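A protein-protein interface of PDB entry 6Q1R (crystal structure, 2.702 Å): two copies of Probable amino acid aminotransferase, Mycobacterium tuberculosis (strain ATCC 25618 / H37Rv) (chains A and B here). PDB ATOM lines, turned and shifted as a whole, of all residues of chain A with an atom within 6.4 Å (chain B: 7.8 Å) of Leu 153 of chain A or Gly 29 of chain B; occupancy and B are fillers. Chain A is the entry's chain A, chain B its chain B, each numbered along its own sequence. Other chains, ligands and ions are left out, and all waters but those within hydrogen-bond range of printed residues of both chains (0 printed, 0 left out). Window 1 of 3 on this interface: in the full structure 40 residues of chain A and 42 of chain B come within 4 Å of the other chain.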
ATOM      1  N   LEU A  24      -5.323  29.414 -15.886  1.00  0.00           N
ATOM      2  CA  LEU A  24      -4.670  30.203 -16.924  1.00  0.00           C
ATOM      3  C   LEU A  24      -4.319  29.395 -18.168  1.00  0.00           C
ATOM      4  O   LEU A  24      -3.988  29.997 -19.195  1.00  0.00           O
ATOM      5  CB  LEU A  24      -3.411  30.861 -16.358  1.00  0.00           C
ATOM      6  CG  LEU A  24      -3.651  32.016 -15.380  1.00  0.00           C
ATOM      7  CD1 LEU A  24      -2.360  32.389 -14.683  1.00  0.00           C
ATOM      8  CD2 LEU A  24      -4.245  33.219 -16.086  1.00  0.00           C
ATOM      9  N   ALA A  25      -4.357  28.058 -18.104  1.00  0.00           N
ATOM     10  CA  ALA A  25      -4.122  27.261 -19.307  1.00  0.00           C
ATOM     11  C   ALA A  25      -5.253  27.421 -20.312  1.00  0.00           C
ATOM     12  O   ALA A  25      -5.016  27.413 -21.526  1.00  0.00           O
ATOM     13  CB  ALA A  25      -3.951  25.787 -18.944  1.00  0.00           C
ATOM     14  N   ALA A  26      -6.483  27.575 -19.828  1.00  0.00           N
ATOM     15  CA  ALA A  26      -7.641  27.767 -20.686  1.00  0.00           C
ATOM     16  C   ALA A  26      -8.027  29.227 -20.846  1.00  0.00           C
ATOM     17  O   ALA A  26      -8.544  29.605 -21.900  1.00  0.00           O
ATOM     18  CB  ALA A  26      -8.839  26.987 -20.140  1.00  0.00           C
ATOM     19  N   ARG A  28      -5.918  31.938 -20.723  1.00  0.00           N
ATOM     20  CA  ARG A  28      -4.947  32.732 -21.465  1.00  0.00           C
ATOM     21  C   ARG A  28      -3.893  31.893 -22.179  1.00  0.00           C
ATOM     22  O   ARG A  28      -2.965  32.464 -22.763  1.00  0.00           O
ATOM     23  CB  ARG A  28      -4.288  33.752 -20.523  1.00  0.00           C
ATOM     24  CG  ARG A  28      -5.140  35.006 -20.377  1.00  0.00           C
ATOM     25  CD  ARG A  28      -4.419  36.176 -19.744  1.00  0.00           C
ATOM     26  NE  ARG A  28      -5.380  37.126 -19.182  1.00  0.00           N
ATOM     27  CZ  ARG A  28      -5.610  37.287 -17.879  1.00  0.00           C
ATOM     28  NH1 ARG A  28      -4.940  36.568 -16.988  1.00  0.00           N
ATOM     29  NH2 ARG A  28      -6.509  38.172 -17.466  1.00  0.00           N
ATOM     30  N   GLY A  29      -4.011  30.570 -22.173  1.00  0.00           N
ATOM     31  CA  GLY A  29      -2.998  29.730 -22.790  1.00  0.00           C
ATOM     32  C   GLY A  29      -1.635  29.853 -22.154  1.00  0.00           C
ATOM     33  O   GLY A  29      -0.625  29.572 -22.807  1.00  0.00           O
ATOM     34  N   ASP A  30      -1.580  30.232 -20.877  1.00  0.00           N
ATOM     35  CA  ASP A  30      -0.327  30.551 -20.192  1.00  0.00           C
ATOM     36  C   ASP A  30       0.240  29.269 -19.598  1.00  0.00           C
ATOM     37  O   ASP A  30      -0.069  28.888 -18.469  1.00  0.00           O
ATOM     38  CB  ASP A  30      -0.574  31.609 -19.123  1.00  0.00           C
ATOM     39  CG  ASP A  30       0.672  32.389 -18.772  1.00  0.00           C
ATOM     40  OD1 ASP A  30       1.697  32.210 -19.460  1.00  0.00           O
ATOM     41  OD2 ASP A  30       0.619  33.198 -17.823  1.00  0.00           O
ATOM     42  N   GLY A  31       1.100  28.605 -20.357  1.00  0.00           N
ATOM     43  CA  GLY A  31       1.697  27.374 -19.878  1.00  0.00           C
ATOM     44  C   GLY A  31       2.570  26.768 -20.948  1.00  0.00           C
ATOM     45  O   GLY A  31       2.699  27.300 -22.055  1.00  0.00           O
ATOM     46  N   VAL A  32       3.188  25.641 -20.593  1.00  0.00           N
ATOM     47  CA  VAL A  32       4.071  24.897 -21.482  1.00  0.00           C
ATOM     48  C   VAL A  32       3.631  23.443 -21.500  1.00  0.00           C
ATOM     49  O   VAL A  32       2.904  22.980 -20.618  1.00  0.00           O
ATOM     50  CB  VAL A  32       5.553  24.991 -21.063  1.00  0.00           C
ATOM     51  CG1 VAL A  32       6.010  26.441 -21.029  1.00  0.00           C
ATOM     52  CG2 VAL A  32       5.753  24.325 -19.716  1.00  0.00           C
ATOM     53  N   PHE A  33       4.065  22.723 -22.533  1.00  0.00           N
ATOM     54  CA  PHE A  33       3.719  21.316 -22.659  1.00  0.00           C
ATOM     55  C   PHE A  33       4.819  20.574 -23.408  1.00  0.00           C
ATOM     56  O   PHE A  33       5.716  21.173 -24.006  1.00  0.00           O
ATOM     57  CB  PHE A  33       2.358  21.138 -23.347  1.00  0.00           C
ATOM     58  CG  PHE A  33       2.419  21.196 -24.845  1.00  0.00           C
ATOM     59  CD1 PHE A  33       2.396  22.412 -25.505  1.00  0.00           C
ATOM     60  CD2 PHE A  33       2.489  20.032 -25.594  1.00  0.00           C
ATOM     61  CE1 PHE A  33       2.451  22.468 -26.885  1.00  0.00           C
ATOM     62  CE2 PHE A  33       2.543  20.079 -26.972  1.00  0.00           C
ATOM     63  CZ  PHE A  33       2.524  21.300 -27.620  1.00  0.00           C
ATOM     64  N   MET A  60       9.300  31.077 -19.744  1.00  0.00           N
ATOM     65  CA  MET A  60       7.945  31.467 -19.383  1.00  0.00           C
ATOM     66  C   MET A  60       7.827  31.942 -17.942  1.00  0.00           C
ATOM     67  O   MET A  60       6.711  32.207 -17.480  1.00  0.00           O
ATOM     68  CB  MET A  60       6.996  30.289 -19.617  1.00  0.00           C
ATOM     69  CG  MET A  60       6.710  30.022 -21.075  1.00  0.00           C
ATOM     70  SD  MET A  60       5.463  31.154 -21.701  1.00  0.00           S
ATOM     71  CE  MET A  60       3.976  30.468 -20.969  1.00  0.00           C
ATOM     72  N   LEU A  93       2.585  16.144 -21.290  1.00  0.00           N
ATOM     73  CA  LEU A  93       2.737  16.744 -19.967  1.00  0.00           C
ATOM     74  C   LEU A  93       2.286  18.195 -20.022  1.00  0.00           C
ATOM     75  O   LEU A  93       2.823  18.980 -20.803  1.00  0.00           O
ATOM     76  CB  LEU A  93       4.187  16.674 -19.481  1.00  0.00           C
ATOM     77  CG  LEU A  93       5.029  15.391 -19.454  1.00  0.00           C
ATOM     78  CD1 LEU A  93       5.230  14.754 -20.819  1.00  0.00           C
ATOM     79  CD2 LEU A  93       6.381  15.681 -18.818  1.00  0.00           C
ATOM     80  N   ILE A  94       1.303  18.547 -19.200  1.00  0.00           N
ATOM     81  CA  ILE A  94       0.720  19.883 -19.196  1.00  0.00           C
ATOM     82  C   ILE A  94       1.165  20.602 -17.932  1.00  0.00           C
ATOM     83  O   ILE A  94       1.006  20.078 -16.823  1.00  0.00           O
ATOM     84  CB  ILE A  94      -0.813  19.829 -19.278  1.00  0.00           C
ATOM     85  CG1 ILE A  94      -1.258  18.915 -20.426  1.00  0.00           C
ATOM     86  CG2 ILE A  94      -1.369  21.235 -19.441  1.00  0.00           C
ATOM     87  CD1 ILE A  94      -0.700  19.302 -21.779  1.00  0.00           C
ATOM     88  N   TYR A  95       1.730  21.799 -18.102  1.00  0.00           N
ATOM     89  CA  TYR A  95       2.329  22.570 -17.011  1.00  0.00           C
ATOM     90  C   TYR A  95       1.961  24.039 -17.197  1.00  0.00           C
ATOM     91  O   TYR A  95       2.632  24.763 -17.939  1.00  0.00           O
ATOM     92  CB  TYR A  95       3.843  22.362 -16.981  1.00  0.00           C
ATOM     93  CG  TYR A  95       4.562  22.998 -15.810  1.00  0.00           C
ATOM     94  CD1 TYR A  95       4.038  22.951 -14.526  1.00  0.00           C
ATOM     95  CD2 TYR A  95       5.790  23.622 -15.994  1.00  0.00           C
ATOM     96  CE1 TYR A  95       4.705  23.536 -13.464  1.00  0.00           C
ATOM     97  CE2 TYR A  95       6.465  24.202 -14.941  1.00  0.00           C
ATOM     98  CZ  TYR A  95       5.922  24.158 -13.681  1.00  0.00           C
ATOM     99  OH  TYR A  95       6.608  24.740 -12.639  1.00  0.00           O
ATOM    100  N   SER A  96       0.904  24.476 -16.514  1.00  0.00           N
ATOM    101  CA  SER A  96       0.386  25.833 -16.620  1.00  0.00           C
ATOM    102  C   SER A  96       0.757  26.641 -15.386  1.00  0.00           C
ATOM    103  O   SER A  96       1.170  26.099 -14.356  1.00  0.00           O
ATOM    104  CB  SER A  96      -1.133  25.833 -16.786  1.00  0.00           C
ATOM    105  OG  SER A  96      -1.764  26.062 -15.537  1.00  0.00           O
ATOM    106  N   LYS A 151       7.883  25.674 -26.069  1.00  0.00           N
ATOM    107  CA  LYS A 151       6.728  24.853 -26.436  1.00  0.00           C
ATOM    108  C   LYS A 151       5.582  25.260 -25.516  1.00  0.00           C
ATOM    109  O   LYS A 151       5.369  24.676 -24.455  1.00  0.00           O
ATOM    110  CB  LYS A 151       7.062  23.368 -26.330  1.00  0.00           C
ATOM    111  CG  LYS A 151       6.190  22.459 -27.199  1.00  0.00           C
ATOM    112  CD  LYS A 151       6.733  21.027 -27.252  1.00  0.00           C
ATOM    113  CE  LYS A 151       6.021  20.178 -28.299  1.00  0.00           C
ATOM    114  NZ  LYS A 151       6.511  20.586 -29.644  1.00  0.00           N
ATOM    115  N   THR A 152       4.838  26.283 -25.922  1.00  0.00           N
ATOM    116  CA  THR A 152       3.773  26.825 -25.091  1.00  0.00           C
ATOM    117  C   THR A 152       2.426  26.190 -25.432  1.00  0.00           C
ATOM    118  O   THR A 152       2.245  25.561 -26.476  1.00  0.00           O
ATOM    119  CB  THR A 152       3.671  28.343 -25.258  1.00  0.00           C
ATOM    120  OG1 THR A 152       3.095  28.645 -26.538  1.00  0.00           O
ATOM    121  CG2 THR A 152       5.045  29.001 -25.156  1.00  0.00           C
ATOM    122  N   LEU A 153       1.462  26.393 -24.534  1.00  0.00           N
ATOM    123  CA  LEU A 153       0.088  25.962 -24.745  1.00  0.00           C
ATOM    124  C   LEU A 153      -0.671  26.868 -25.701  1.00  0.00           C
ATOM    125  O   LEU A 153      -1.873  26.666 -25.892  1.00  0.00           O
ATOM    126  CB  LEU A 153      -0.664  25.909 -23.414  1.00  0.00           C
ATOM    127  CG  LEU A 153      -0.257  24.831 -22.419  1.00  0.00           C
ATOM    128  CD1 LEU A 153      -0.983  25.035 -21.095  1.00  0.00           C
ATOM    129  CD2 LEU A 153      -0.535  23.455 -22.998  1.00  0.00           C
ATOM    130  N   SER A 154      -0.019  27.877 -26.277  1.00  0.00           N
ATOM    131  CA  SER A 154      -0.681  28.809 -27.189  1.00  0.00           C
ATOM    132  C   SER A 154      -0.420  28.384 -28.631  1.00  0.00           C
ATOM    133  O   SER A 154       0.429  28.940 -29.332  1.00  0.00           O
ATOM    134  CB  SER A 154      -0.220  30.232 -26.913  1.00  0.00           C
ATOM    135  OG  SER A 154      -0.684  30.664 -25.648  1.00  0.00           O
ATOM    136  N   TYR A 155      -1.192  27.391 -29.085  1.00  0.00           N
ATOM    137  CA  TYR A 155      -1.044  26.828 -30.424  1.00  0.00           C
ATOM    138  C   TYR A 155      -2.211  27.193 -31.338  1.00  0.00           C
ATOM    139  O   TYR A 155      -2.420  26.531 -32.361  1.00  0.00           O
ATOM    140  CB  TYR A 155      -0.856  25.307 -30.358  1.00  0.00           C
ATOM    141  CG  TYR A 155       0.607  24.905 -30.274  1.00  0.00           C
ATOM    142  CD1 TYR A 155       1.519  25.703 -29.595  1.00  0.00           C
ATOM    143  CD2 TYR A 155       1.083  23.749 -30.888  1.00  0.00           C
ATOM    144  CE1 TYR A 155       2.859  25.364 -29.511  1.00  0.00           C
ATOM    145  CE2 TYR A 155       2.433  23.397 -30.812  1.00  0.00           C
ATOM    146  CZ  TYR A 155       3.315  24.213 -30.119  1.00  0.00           C
ATOM    147  OH  TYR A 155       4.656  23.900 -30.022  1.00  0.00           O
ATOM    148  N   ALA A 156      -2.967  28.240 -31.006  1.00  0.00           N
ATOM    149  CA  ALA A 156      -4.115  28.616 -31.828  1.00  0.00           C
ATOM    150  C   ALA A 156      -3.695  28.900 -33.265  1.00  0.00           C
ATOM    151  O   ALA A 156      -4.410  28.546 -34.210  1.00  0.00           O
ATOM    152  CB  ALA A 156      -4.826  29.829 -31.231  1.00  0.00           C
ATOM    153  N   ASP B  23      -9.632  19.485 -22.688  1.00  0.00           N
ATOM    154  CA  ASP B  23     -10.294  20.612 -23.330  1.00  0.00           C
ATOM    155  C   ASP B  23      -9.276  21.407 -24.137  1.00  0.00           C
ATOM    156  O   ASP B  23      -8.221  21.788 -23.620  1.00  0.00           O
ATOM    157  CB  ASP B  23     -10.964  21.497 -22.278  1.00  0.00           C
ATOM    158  CG  ASP B  23     -11.927  22.511 -22.883  1.00  0.00           C
ATOM    159  OD1 ASP B  23     -11.477  23.384 -23.656  1.00  0.00           O
ATOM    160  OD2 ASP B  23     -13.142  22.430 -22.588  1.00  0.00           O
ATOM    161  N   LEU B  24      -9.596  21.660 -25.410  1.00  0.00           N
ATOM    162  CA  LEU B  24      -8.649  22.306 -26.316  1.00  0.00           C
ATOM    163  C   LEU B  24      -8.314  23.736 -25.913  1.00  0.00           C
ATOM    164  O   LEU B  24      -7.336  24.289 -26.426  1.00  0.00           O
ATOM    165  CB  LEU B  24      -9.187  22.282 -27.746  1.00  0.00           C
ATOM    166  CG  LEU B  24      -9.116  20.906 -28.402  1.00  0.00           C
ATOM    167  CD1 LEU B  24      -9.909  20.875 -29.693  1.00  0.00           C
ATOM    168  CD2 LEU B  24      -7.666  20.546 -28.651  1.00  0.00           C
ATOM    169  N   ALA B  25      -9.098  24.353 -25.026  1.00  0.00           N
ATOM    170  CA  ALA B  25      -8.725  25.673 -24.528  1.00  0.00           C
ATOM    171  C   ALA B  25      -7.473  25.597 -23.672  1.00  0.00           C
ATOM    172  O   ALA B  25      -6.666  26.533 -23.664  1.00  0.00           O
ATOM    173  CB  ALA B  25      -9.867  26.290 -23.724  1.00  0.00           C
ATOM    174  N   ALA B  26      -7.291  24.493 -22.955  1.00  0.00           N
ATOM    175  CA  ALA B  26      -6.132  24.308 -22.102  1.00  0.00           C
ATOM    176  C   ALA B  26      -5.012  23.521 -22.763  1.00  0.00           C
ATOM    177  O   ALA B  26      -3.841  23.765 -22.459  1.00  0.00           O
ATOM    178  CB  ALA B  26      -6.546  23.602 -20.809  1.00  0.00           C
ATOM    179  N   VAL B  27      -5.331  22.585 -23.652  1.00  0.00           N
ATOM    180  CA  VAL B  27      -4.286  21.772 -24.267  1.00  0.00           C
ATOM    181  C   VAL B  27      -3.599  22.526 -25.403  1.00  0.00           C
ATOM    182  O   VAL B  27      -2.388  22.386 -25.611  1.00  0.00           O
ATOM    183  CB  VAL B  27      -4.872  20.423 -24.717  1.00  0.00           C
ATOM    184  CG1 VAL B  27      -3.856  19.621 -25.514  1.00  0.00           C
ATOM    185  CG2 VAL B  27      -5.314  19.642 -23.498  1.00  0.00           C
ATOM    186  N   ARG B  28      -4.348  23.349 -26.142  1.00  0.00           N
ATOM    187  CA  ARG B  28      -3.822  24.067 -27.297  1.00  0.00           C
ATOM    188  C   ARG B  28      -4.164  25.550 -27.343  1.00  0.00           C
ATOM    189  O   ARG B  28      -3.776  26.218 -28.308  1.00  0.00           O
ATOM    190  CB  ARG B  28      -4.317  23.440 -28.619  1.00  0.00           C
ATOM    191  CG  ARG B  28      -3.395  22.427 -29.300  1.00  0.00           C
ATOM    192  CD  ARG B  28      -3.205  21.137 -28.564  1.00  0.00           C
ATOM    193  NE  ARG B  28      -1.993  20.454 -29.011  1.00  0.00           N
ATOM    194  CZ  ARG B  28      -1.948  19.601 -30.028  1.00  0.00           C
ATOM    195  NH1 ARG B  28      -3.054  19.331 -30.714  1.00  0.00           N
ATOM    196  NH2 ARG B  28      -0.802  19.022 -30.362  1.00  0.00           N
ATOM    197  N   GLY B  29      -4.828  26.096 -26.328  1.00  0.00           N
ATOM    198  CA  GLY B  29      -5.232  27.491 -26.412  1.00  0.00           C
ATOM    199  C   GLY B  29      -6.167  27.755 -27.569  1.00  0.00           C
ATOM    200  O   GLY B  29      -6.219  28.878 -28.082  1.00  0.00           O
ATOM    201  N   ASP B  30      -6.907  26.732 -27.999  1.00  0.00           N
ATOM    202  CA  ASP B  30      -7.736  26.780 -29.202  1.00  0.00           C
ATOM    203  C   ASP B  30      -9.119  27.285 -28.807  1.00  0.00           C
ATOM    204  O   ASP B  30      -9.989  26.521 -28.389  1.00  0.00           O
ATOM    205  CB  ASP B  30      -7.786  25.401 -29.848  1.00  0.00           C
ATOM    206  CG  ASP B  30      -8.104  25.454 -31.326  1.00  0.00           C
ATOM    207  OD1 ASP B  30      -8.223  24.377 -31.943  1.00  0.00           O
ATOM    208  OD2 ASP B  30      -8.167  26.564 -31.889  1.00  0.00           O
ATOM    209  N   GLY B  31      -9.318  28.592 -28.921  1.00  0.00           N
ATOM    210  CA  GLY B  31     -10.606  29.179 -28.602  1.00  0.00           C
ATOM    211  C   GLY B  31     -10.533  30.684 -28.722  1.00  0.00           C
ATOM    212  O   GLY B  31      -9.476  31.258 -28.997  1.00  0.00           O
ATOM    213  N   VAL B  32     -11.682  31.326 -28.503  1.00  0.00           N
ATOM    214  CA  VAL B  32     -11.784  32.778 -28.557  1.00  0.00           C
ATOM    215  C   VAL B  32     -12.447  33.270 -27.278  1.00  0.00           C
ATOM    216  O   VAL B  32     -13.150  32.526 -26.591  1.00  0.00           O
ATOM    217  CB  VAL B  32     -12.569  33.270 -29.793  1.00  0.00           C
ATOM    218  CG1 VAL B  32     -11.918  32.777 -31.069  1.00  0.00           C
ATOM    219  CG2 VAL B  32     -14.012  32.818 -29.721  1.00  0.00           C
ATOM    220  N   MET B  60     -11.839  31.322 -36.562  1.00  0.00           N
ATOM    221  CA  MET B  60     -11.283  30.154 -35.900  1.00  0.00           C
ATOM    222  C   MET B  60     -12.011  28.864 -36.252  1.00  0.00           C
ATOM    223  O   MET B  60     -11.752  27.833 -35.623  1.00  0.00           O
ATOM    224  CB  MET B  60     -11.300  30.371 -34.387  1.00  0.00           C
ATOM    225  CG  MET B  60     -10.234  31.335 -33.923  1.00  0.00           C
ATOM    226  SD  MET B  60      -8.634  30.525 -33.791  1.00  0.00           S
ATOM    227  CE  MET B  60      -8.874  29.582 -32.288  1.00  0.00           C
ATOM    228  N   TYR B  95     -14.963  30.708 -25.090  1.00  0.00           N
ATOM    229  CA  TYR B  95     -15.578  29.950 -26.181  1.00  0.00           C
ATOM    230  C   TYR B  95     -14.493  29.082 -26.810  1.00  0.00           C
ATOM    231  O   TYR B  95     -13.718  29.553 -27.647  1.00  0.00           O
ATOM    232  CB  TYR B  95     -16.219  30.886 -27.201  1.00  0.00           C
ATOM    233  CG  TYR B  95     -17.078  30.183 -28.221  1.00  0.00           C
ATOM    234  CD1 TYR B  95     -17.937  29.162 -27.837  1.00  0.00           C
ATOM    235  CD2 TYR B  95     -17.057  30.555 -29.559  1.00  0.00           C
ATOM    236  CE1 TYR B  95     -18.737  28.514 -28.757  1.00  0.00           C
ATOM    237  CE2 TYR B  95     -17.861  29.910 -30.492  1.00  0.00           C
ATOM    238  CZ  TYR B  95     -18.699  28.889 -30.079  1.00  0.00           C
ATOM    239  OH  TYR B  95     -19.504  28.234 -30.981  1.00  0.00           O
ATOM    240  N   SER B  96     -14.445  27.820 -26.402  1.00  0.00           N
ATOM    241  CA  SER B  96     -13.421  26.880 -26.828  1.00  0.00           C
ATOM    242  C   SER B  96     -13.969  25.903 -27.862  1.00  0.00           C
ATOM    243  O   SER B  96     -15.179  25.770 -28.056  1.00  0.00           O
ATOM    244  CB  SER B  96     -12.878  26.116 -25.614  1.00  0.00           C
ATOM    245  OG  SER B  96     -12.314  24.868 -25.984  1.00  0.00           O
ATOM    246  N   ARG B  97     -13.046  25.210 -28.530  1.00  0.00           N
ATOM    247  CA  ARG B  97     -13.417  24.186 -29.495  1.00  0.00           C
ATOM    248  C   ARG B  97     -14.028  22.961 -28.828  1.00  0.00           C
ATOM    249  O   ARG B  97     -14.594  22.111 -29.523  1.00  0.00           O
ATOM    250  CB  ARG B  97     -12.196  23.789 -30.329  1.00  0.00           C
ATOM    251  CG  ARG B  97     -12.537  23.072 -31.635  1.00  0.00           C
ATOM    252  CD  ARG B  97     -11.334  22.975 -32.561  1.00  0.00           C
ATOM    253  NE  ARG B  97     -10.686  24.272 -32.732  1.00  0.00           N
ATOM    254  CZ  ARG B  97     -11.009  25.156 -33.672  1.00  0.00           C
ATOM    255  NH1 ARG B  97     -11.975  24.888 -34.543  1.00  0.00           N
ATOM    256  NH2 ARG B  97     -10.363  26.312 -33.740  1.00  0.00           N
ATOM    257  N   ILE B 147      -4.361  34.843 -38.350  1.00  0.00           N
ATOM    258  CA  ILE B 147      -5.513  35.219 -37.525  1.00  0.00           C
ATOM    259  C   ILE B 147      -5.169  36.314 -36.519  1.00  0.00           C
ATOM    260  O   ILE B 147      -5.610  36.279 -35.365  1.00  0.00           O
ATOM    261  CB  ILE B 147      -6.125  33.983 -36.828  1.00  0.00           C
ATOM    262  CG1 ILE B 147      -5.147  33.330 -35.843  1.00  0.00           C
ATOM    263  CG2 ILE B 147      -6.609  32.969 -37.861  1.00  0.00           C
ATOM    264  CD1 ILE B 147      -5.717  32.152 -35.107  1.00  0.00           C
ATOM    265  N   THR B 152      -7.975  35.455 -29.527  1.00  0.00           N
ATOM    266  CA  THR B 152      -7.893  34.040 -29.201  1.00  0.00           C
ATOM    267  C   THR B 152      -7.466  33.838 -27.746  1.00  0.00           C
ATOM    268  O   THR B 152      -6.986  34.755 -27.071  1.00  0.00           O
ATOM    269  CB  THR B 152      -6.918  33.315 -30.134  1.00  0.00           C
ATOM    270  OG1 THR B 152      -5.569  33.672 -29.798  1.00  0.00           O
ATOM    271  CG2 THR B 152      -7.182  33.686 -31.585  1.00  0.00           C
ATOM    272  N   LEU B 153      -7.644  32.605 -27.271  1.00  0.00           N
ATOM    273  CA  LEU B 153      -7.211  32.196 -25.939  1.00  0.00           C
ATOM    274  C   LEU B 153      -5.709  31.959 -25.851  1.00  0.00           C
ATOM    275  O   LEU B 153      -5.229  31.538 -24.794  1.00  0.00           O
ATOM    276  CB  LEU B 153      -7.956  30.928 -25.511  1.00  0.00           C
ATOM    277  CG  LEU B 153      -9.447  31.092 -25.223  1.00  0.00           C
ATOM    278  CD1 LEU B 153     -10.119  29.741 -24.991  1.00  0.00           C
ATOM    279  CD2 LEU B 153      -9.645  32.007 -24.026  1.00  0.00           C
ATOM    280  N   SER B 154      -4.963  32.202 -26.928  1.00  0.00           N
ATOM    281  CA  SER B 154      -3.517  31.990 -26.948  1.00  0.00           C
ATOM    282  C   SER B 154      -2.827  33.325 -26.669  1.00  0.00           C
ATOM    283  O   SER B 154      -2.353  34.021 -27.566  1.00  0.00           O
ATOM    284  CB  SER B 154      -3.093  31.380 -28.274  1.00  0.00           C
ATOM    285  OG  SER B 154      -3.604  30.064 -28.389  1.00  0.00           O
ATOM    286  N   TYR B 155      -2.748  33.655 -25.380  1.00  0.00           N
ATOM    287  CA  TYR B 155      -2.234  34.929 -24.893  1.00  0.00           C
ATOM    288  C   TYR B 155      -0.868  34.800 -24.231  1.00  0.00           C
ATOM    289  O   TYR B 155      -0.449  35.722 -23.526  1.00  0.00           O
ATOM    290  CB  TYR B 155      -3.225  35.509 -23.880  1.00  0.00           C
ATOM    291  CG  TYR B 155      -3.720  36.913 -24.132  1.00  0.00           C
ATOM    292  CD1 TYR B 155      -3.160  37.994 -23.463  1.00  0.00           C
ATOM    293  CD2 TYR B 155      -4.783  37.156 -25.001  1.00  0.00           C
ATOM    294  CE1 TYR B 155      -3.619  39.283 -23.672  1.00  0.00           C
ATOM    295  CE2 TYR B 155      -5.252  38.443 -25.216  1.00  0.00           C
ATOM    296  CZ  TYR B 155      -4.667  39.503 -24.548  1.00  0.00           C
ATOM    297  OH  TYR B 155      -5.125  40.786 -24.751  1.00  0.00           O
ATOM    298  N   ALA B 156      -0.162  33.686 -24.443  1.00  0.00           N
ATOM    299  CA  ALA B 156       1.109  33.466 -23.757  1.00  0.00           C
ATOM    300  C   ALA B 156       2.150  34.521 -24.113  1.00  0.00           C
ATOM    301  O   ALA B 156       2.867  35.013 -23.232  1.00  0.00           O
ATOM    302  CB  ALA B 156       1.642  32.073 -24.080  1.00  0.00           C
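Ala 26 of chain B touches its own counterpart, Ala 26 of chain A. Gly 29 of chain A touches Ala 156 of chain B, and with the chains exchanged Ala 156 of chain A touches Gly 29 of chain B. Ser 154 of chain A touches Tyr 155 of chain B, and with the chains exchanged Tyr 155 of chain A touches Ser 154 of chain B.
Along chain B the printed residues that touch a printed residue of chain A span positions 25 to 156. Printed residues of chain A that touch a printed residue of chain B: Ala 25, Ala 26, Arg 28, Gly 29, Leu 153, Ser 154, Tyr 155 and Ala 156. Hydrophobic or aromatic side chains of chain A that line the printed part of chain B: Ala 25, Ala 26, Leu 153, Tyr 155 and Ala 156. Among the printed residues, no Asp or Glu carboxylate lies within 4 Å of a Lys or Arg side-chain nitrogen of the other chain.
Printed residues of chain B within 4 Å of Tyr 155 of chain A: Arg 28 and Ser 154. Printed residues of chain B within 4 Å of Ala 156 of chain A: Arg 28 (3.5 Å), Gly 29 (3.6 Å), Ile 147 (3.9 Å) and Ser 154 (3.1 Å). Printed residues of chain A within 4 Å of Ala 25 of chain B: Ala 25 (2.8 Å) and Ala 26 (3.4 Å). Gly 29 of chain B touches just these residues of chain A: Leu 153 (3.0 Å) and Ala 156 (3.6 Å). Printed residues of chain A within 4 Å of Ile 147 of chain B: Ala 156. The nearest residue of chain B that does not touch Leu 153 of chain A is Ser 154 of chain B (4.6 Å). The nearest printed residue of chain A that does not touch Ala 26 of chain B is Ile 94 of chain A (4.6 Å).
Among the printed residues, pairs that only touch across the chains: Ala 25 of chain A with Ala 26 of chain B, Leu 153 of chain A with Ala 26 of chain B, Ala 26 of chain A with Ala 25 of chain B, Leu 153 of chain A with Val 27 of chain B, Ser 154 of chain A with Ser 154 of chain B, Ala 26 of chain A with Leu 153 of chain B, Ala 156 of chain A with Gly 29 of chain B, Gly 29 of chain A with Ala 156 of chain B, Ser 154 of chain A with Tyr 155 of chain B, Tyr 155 of chain A with Ser 154 of chain B, Ala 156 of chain A with Ile 147 of chain B and Ala 26 of chain A with Ala 26 of chain B.
The backbone carbonyl oxygen (O) of Arg 28 of chain A lies within hydrogen-bond range of the backbone NH (N) of Tyr 155 of chain B (2.9 Å). The backbone NH (N) of Ala 156 of chain B is in hydrogen-bond range of the backbone carbonyl oxygen (O) of Arg 28 of chain A (3.5 Å). N of Gly 29 of chain A is in hydrogen-bond range of O of Leu 153 of chain B, 3.0 Å away. O of Leu 153 of chain A sits at hydrogen-bond distance from N of Gly 29 of chain B, at 3.0 Å. The side-chain hydroxyl of Ser 154 of chain A lies close to the backbone NH of Ala 156 of chain B, at 3.3 Å. N of Tyr 155 of chain A sits at hydrogen-bond distance from O of Arg 28 of chain B, at 2.9 Å. N of Ala 156 of chain A sits at hydrogen-bond distance from O of Arg 28 of chain B. The backbone NH of Ala 156 of chain A lies close to the side-chain hydroxyl of Ser 154 of chain B (3.3 Å). O of Ala 25 of chain A lies close to O of Ala 25 of chain B (2.8 Å). O of Leu 153 of chain B sits close to O of Arg 28 of chain A (3.2 Å). The backbone carbonyl oxygen of Leu 153 of chain A lies close to the backbone carbonyl oxygen of Arg 28 of chain B, at 3.1 Å.
The backbone NH (N) of Leu 153 of chain A lies within hydrogen-bond range of the backbone carbonyl oxygen (O) of Gly 31 of chain A, 2.9 Å away. The backbone carbonyl oxygen of Gly 31 of chain B lies within hydrogen-bond range of the backbone NH of Leu 153 of chain B (2.9 Å).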
